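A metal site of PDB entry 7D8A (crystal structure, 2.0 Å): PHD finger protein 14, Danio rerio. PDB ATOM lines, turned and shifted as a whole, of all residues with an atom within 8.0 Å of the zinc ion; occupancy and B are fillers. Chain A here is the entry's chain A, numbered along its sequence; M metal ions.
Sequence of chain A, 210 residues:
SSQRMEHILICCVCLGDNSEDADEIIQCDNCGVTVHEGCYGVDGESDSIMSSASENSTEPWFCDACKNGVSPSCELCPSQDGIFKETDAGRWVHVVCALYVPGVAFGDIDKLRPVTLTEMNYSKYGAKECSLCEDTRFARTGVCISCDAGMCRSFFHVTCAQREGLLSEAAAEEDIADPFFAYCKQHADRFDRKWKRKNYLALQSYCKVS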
ATOM      1  N   SER A 146     -19.177 -31.871 -10.092  1.00  0.00           N
ATOM      2  CA  SER A 146     -19.415 -31.402  -8.741  1.00  0.00           C
ATOM      3  C   SER A 146     -18.151 -30.818  -8.110  1.00  0.00           C
ATOM      4  O   SER A 146     -17.031 -30.971  -8.591  1.00  0.00           O
ATOM      5  CB  SER A 146     -19.984 -32.506  -7.860  1.00  0.00           C
ATOM      6  OG  SER A 146     -19.040 -33.539  -7.687  1.00  0.00           O
ATOM      7  N   CYS A 147     -18.362 -30.105  -6.997  1.00  0.00           N
ATOM      8  CA  CYS A 147     -17.273 -29.693  -6.136  1.00  0.00           C
ATOM      9  C   CYS A 147     -16.503 -30.923  -5.678  1.00  0.00           C
ATOM     10  O   CYS A 147     -17.081 -31.972  -5.369  1.00  0.00           O
ATOM     11  CB  CYS A 147     -17.830 -28.900  -4.947  1.00  0.00           C
ATOM     12  SG  CYS A 147     -16.592 -28.392  -3.739  1.00  0.00           S
ATOM     13  N   ASP A 148     -15.181 -30.798  -5.645  1.00  0.00           N
ATOM     14  CA  ASP A 148     -14.318 -31.909  -5.251  1.00  0.00           C
ATOM     15  C   ASP A 148     -13.844 -31.846  -3.807  1.00  0.00           C
ATOM     16  O   ASP A 148     -12.925 -32.592  -3.455  1.00  0.00           O
ATOM     17  CB  ASP A 148     -13.119 -32.002  -6.190  1.00  0.00           C
ATOM     18  CG  ASP A 148     -13.490 -32.576  -7.544  1.00  0.00           C
ATOM     19  OD1 ASP A 148     -14.137 -33.643  -7.578  1.00  0.00           O
ATOM     20  OD2 ASP A 148     -13.150 -31.955  -8.559  1.00  0.00           O
ATOM     21  N   ALA A 149     -14.412 -30.963  -2.980  1.00  0.00           N
ATOM     22  CA  ALA A 149     -14.041 -30.865  -1.559  1.00  0.00           C
ATOM     23  C   ALA A 149     -14.877 -31.852  -0.741  1.00  0.00           C
ATOM     24  O   ALA A 149     -16.112 -31.769  -0.750  1.00  0.00           O
ATOM     25  CB  ALA A 149     -14.245 -29.451  -1.016  1.00  0.00           C
ATOM     26  N   GLY A 150     -14.195 -32.739  -0.021  1.00  0.00           N
ATOM     27  CA  GLY A 150     -14.882 -33.693   0.833  1.00  0.00           C
ATOM     28  C   GLY A 150     -16.007 -34.407   0.115  1.00  0.00           C
ATOM     29  O   GLY A 150     -15.841 -34.955  -0.978  1.00  0.00           O
ATOM     30  N   MET A 151     -17.186 -34.387   0.730  1.00  0.00           N
ATOM     31  CA  MET A 151     -18.393 -34.938   0.141  1.00  0.00           C
ATOM     32  C   MET A 151     -19.373 -33.845  -0.263  1.00  0.00           C
ATOM     33  O   MET A 151     -20.582 -34.041  -0.222  1.00  0.00           O
ATOM     34  CB  MET A 151     -19.044 -35.935   1.107  1.00  0.00           C
ATOM     35  CG  MET A 151     -18.103 -37.045   1.587  1.00  0.00           C
ATOM     36  SD  MET A 151     -17.174 -37.900   0.266  1.00  0.00           S
ATOM     37  CE  MET A 151     -16.376 -39.216   1.187  1.00  0.00           C
ATOM     38  N   CYS A 152     -18.844 -32.665  -0.632  1.00  0.00           N
ATOM     39  CA  CYS A 152     -19.707 -31.557  -1.040  1.00  0.00           C
ATOM     40  C   CYS A 152     -20.468 -31.933  -2.301  1.00  0.00           C
ATOM     41  O   CYS A 152     -19.874 -32.381  -3.287  1.00  0.00           O
ATOM     42  CB  CYS A 152     -18.869 -30.303  -1.281  1.00  0.00           C
ATOM     43  SG  CYS A 152     -19.867 -28.850  -1.696  1.00  0.00           S
ATOM     44  N   ARG A 153     -21.782 -31.743  -2.284  1.00  0.00           N
ATOM     45  CA  ARG A 153     -22.579 -32.116  -3.445  1.00  0.00           C
ATOM     46  C   ARG A 153     -23.160 -30.864  -4.090  1.00  0.00           C
ATOM     47  O   ARG A 153     -24.373 -30.634  -4.054  1.00  0.00           O
ATOM     48  CB  ARG A 153     -23.684 -33.111  -3.038  1.00  0.00           C
ATOM     49  CG  ARG A 153     -23.167 -34.449  -2.540  1.00  0.00           C
ATOM     50  CD  ARG A 153     -21.983 -34.940  -3.379  1.00  0.00           C
ATOM     51  NE  ARG A 153     -22.376 -35.702  -4.567  1.00  0.00           N
ATOM     52  CZ  ARG A 153     -21.622 -35.798  -5.664  1.00  0.00           C
ATOM     53  NH1 ARG A 153     -22.030 -36.507  -6.703  1.00  0.00           N
ATOM     54  NH2 ARG A 153     -20.454 -35.162  -5.719  1.00  0.00           N
ATOM     55  N   SER A 154     -22.283 -30.046  -4.659  1.00  0.00           N
ATOM     56  CA  SER A 154     -22.663 -28.824  -5.355  1.00  0.00           C
ATOM     57  C   SER A 154     -22.313 -29.017  -6.813  1.00  0.00           C
ATOM     58  O   SER A 154     -21.185 -29.410  -7.131  1.00  0.00           O
ATOM     59  CB  SER A 154     -21.942 -27.621  -4.750  1.00  0.00           C
ATOM     60  OG  SER A 154     -22.259 -26.436  -5.445  1.00  0.00           O
ATOM     61  N   PHE A 155     -23.271 -28.782  -7.708  1.00  0.00           N
ATOM     62  CA  PHE A 155     -23.141 -29.195  -9.093  1.00  0.00           C
ATOM     63  C   PHE A 155     -23.153 -27.991 -10.025  1.00  0.00           C
ATOM     64  O   PHE A 155     -23.875 -27.019  -9.778  1.00  0.00           O
ATOM     65  CB  PHE A 155     -24.271 -30.170  -9.496  1.00  0.00           C
ATOM     66  CG  PHE A 155     -24.473 -31.315  -8.534  1.00  0.00           C
ATOM     67  CD1 PHE A 155     -23.516 -32.298  -8.388  1.00  0.00           C
ATOM     68  CD2 PHE A 155     -25.645 -31.419  -7.803  1.00  0.00           C
ATOM     69  CE1 PHE A 155     -23.694 -33.356  -7.510  1.00  0.00           C
ATOM     70  CE2 PHE A 155     -25.842 -32.470  -6.913  1.00  0.00           C
ATOM     71  CZ  PHE A 155     -24.863 -33.444  -6.769  1.00  0.00           C
ATOM     72  N   PHE A 156     -22.348 -28.038 -11.083  1.00  0.00           N
ATOM     73  CA  PHE A 156     -22.351 -26.986 -12.082  1.00  0.00           C
ATOM     74  C   PHE A 156     -21.802 -27.529 -13.394  1.00  0.00           C
ATOM     75  O   PHE A 156     -20.999 -28.460 -13.412  1.00  0.00           O
ATOM     76  CB  PHE A 156     -21.507 -25.772 -11.625  1.00  0.00           C
ATOM     77  CG  PHE A 156     -20.437 -26.125 -10.638  1.00  0.00           C
ATOM     78  CD1 PHE A 156     -19.356 -26.911 -11.024  1.00  0.00           C
ATOM     79  CD2 PHE A 156     -20.527 -25.728  -9.314  1.00  0.00           C
ATOM     80  CE1 PHE A 156     -18.388 -27.275 -10.099  1.00  0.00           C
ATOM     81  CE2 PHE A 156     -19.556 -26.076  -8.379  1.00  0.00           C
ATOM     82  CZ  PHE A 156     -18.481 -26.846  -8.768  1.00  0.00           C
ATOM     83  N   ALA A 182     -12.457 -29.061  -9.377  1.00  0.00           N
ATOM     84  CA  ALA A 182     -13.236 -27.854  -9.176  1.00  0.00           C
ATOM     85  C   ALA A 182     -13.765 -27.817  -7.739  1.00  0.00           C
ATOM     86  O   ALA A 182     -14.095 -28.847  -7.159  1.00  0.00           O
ATOM     87  CB  ALA A 182     -14.409 -27.817 -10.184  1.00  0.00           C
ATOM     88  N   TYR A 183     -13.844 -26.613  -7.169  1.00  0.00           N
ATOM     89  CA  TYR A 183     -14.526 -26.390  -5.898  1.00  0.00           C
ATOM     90  C   TYR A 183     -15.655 -25.409  -6.102  1.00  0.00           C
ATOM     91  O   TYR A 183     -15.567 -24.505  -6.936  1.00  0.00           O
ATOM     92  CB  TYR A 183     -13.565 -25.854  -4.798  1.00  0.00           C
ATOM     93  CG  TYR A 183     -12.369 -26.743  -4.478  1.00  0.00           C
ATOM     94  CD1 TYR A 183     -12.513 -28.127  -4.324  1.00  0.00           C
ATOM     95  CD2 TYR A 183     -11.101 -26.203  -4.322  1.00  0.00           C
ATOM     96  CE1 TYR A 183     -11.421 -28.932  -4.008  1.00  0.00           C
ATOM     97  CE2 TYR A 183      -9.996 -27.000  -4.024  1.00  0.00           C
ATOM     98  CZ  TYR A 183     -10.164 -28.355  -3.869  1.00  0.00           C
ATOM     99  OH  TYR A 183      -9.063 -29.125  -3.554  1.00  0.00           O
ATOM    100  N   CYS A 184     -16.719 -25.569  -5.337  1.00  0.00           N
ATOM    101  CA  CYS A 184     -17.756 -24.543  -5.319  1.00  0.00           C
ATOM    102  C   CYS A 184     -17.212 -23.285  -4.631  1.00  0.00           C
ATOM    103  O   CYS A 184     -16.097 -23.278  -4.105  1.00  0.00           O
ATOM    104  CB  CYS A 184     -19.004 -25.069  -4.621  1.00  0.00           C
ATOM    105  SG  CYS A 184     -18.806 -25.320  -2.828  1.00  0.00           S
ATOM    106  N   LYS A 185     -18.008 -22.199  -4.649  1.00  0.00           N
ATOM    107  CA  LYS A 185     -17.521 -20.945  -4.070  1.00  0.00           C
ATOM    108  C   LYS A 185     -17.262 -21.087  -2.579  1.00  0.00           C
ATOM    109  O   LYS A 185     -16.366 -20.428  -2.044  1.00  0.00           O
ATOM    110  CB  LYS A 185     -18.520 -19.803  -4.282  1.00  0.00           C
ATOM    111  CG  LYS A 185     -18.880 -19.557  -5.754  1.00  0.00           C
ATOM    112  CD  LYS A 185     -19.811 -18.324  -5.885  1.00  0.00           C
ATOM    113  CE  LYS A 185     -20.624 -18.395  -7.174  1.00  0.00           C
ATOM    114  NZ  LYS A 185     -21.840 -17.522  -7.164  1.00  0.00           N
ATOM    115  N   GLN A 186     -18.048 -21.932  -1.902  1.00  0.00           N
ATOM    116  CA  GLN A 186     -17.906 -22.111  -0.467  1.00  0.00           C
ATOM    117  C   GLN A 186     -16.556 -22.728  -0.131  1.00  0.00           C
ATOM    118  O   GLN A 186     -15.962 -22.412   0.920  1.00  0.00           O
ATOM    119  CB  GLN A 186     -19.051 -22.991   0.036  1.00  0.00           C
ATOM    120  CG  GLN A 186     -19.059 -23.270   1.524  1.00  0.00           C
ATOM    121  CD  GLN A 186     -20.253 -24.115   1.933  1.00  0.00           C
ATOM    122  OE1 GLN A 186     -21.199 -24.287   1.161  1.00  0.00           O
ATOM    123  NE2 GLN A 186     -20.207 -24.664   3.149  1.00  0.00           N
ATOM    124  N   HIS A 187     -16.012 -23.552  -1.022  1.00  0.00           N
ATOM    125  CA  HIS A 187     -14.789 -24.286  -0.746  1.00  0.00           C
ATOM    126  C   HIS A 187     -13.613 -23.839  -1.599  1.00  0.00           C
ATOM    127  O   HIS A 187     -12.525 -24.397  -1.479  1.00  0.00           O
ATOM    128  CB  HIS A 187     -15.063 -25.773  -0.916  1.00  0.00           C
ATOM    129  CG  HIS A 187     -16.054 -26.278   0.081  1.00  0.00           C
ATOM    130  ND1 HIS A 187     -17.186 -26.985  -0.268  1.00  0.00           N
ATOM    131  CD2 HIS A 187     -16.076 -26.161   1.426  1.00  0.00           C
ATOM    132  CE1 HIS A 187     -17.865 -27.275   0.824  1.00  0.00           C
ATOM    133  NE2 HIS A 187     -17.220 -26.786   1.871  1.00  0.00           N
ATOM    134  N   ALA A 188     -13.782 -22.800  -2.413  1.00  0.00           N
ATOM    135  CA  ALA A 188     -12.730 -22.414  -3.339  1.00  0.00           C
ATOM    136  C   ALA A 188     -11.595 -21.660  -2.631  1.00  0.00           C
ATOM    137  O   ALA A 188     -11.740 -21.148  -1.508  1.00  0.00           O
ATOM    138  CB  ALA A 188     -13.297 -21.570  -4.478  1.00  0.00           C
HETATM  139 ZN    ZN M   1     -18.082 -27.388  -2.234  1.00  0.00          ZN
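The side-chain sulfur of Cys 184 lies close to the backbone NH of Gln 186.
SG of Cys 147 lies close to N of Ala 149, 3.5 Å away.
The backbone NH (N) of Cys 147 is in hydrogen-bond range of the backbone carbonyl oxygen (O) of Ser 154, at 2.9 Å.
The zinc ion is bound by a ring nitrogen (ND1) of His 187 (2.2 Å), the side-chain sulfur of Cys 184 (2.3 Å), the side-chain sulfur of Cys 147 (2.3 Å) and the side-chain sulfur of Cys 152 (2.4 Å).
The zinc ion has four donor atoms within binding distance.
Within 4 Å of the zinc ion: Cys 147, Cys 152, Cys 184 and His 187.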
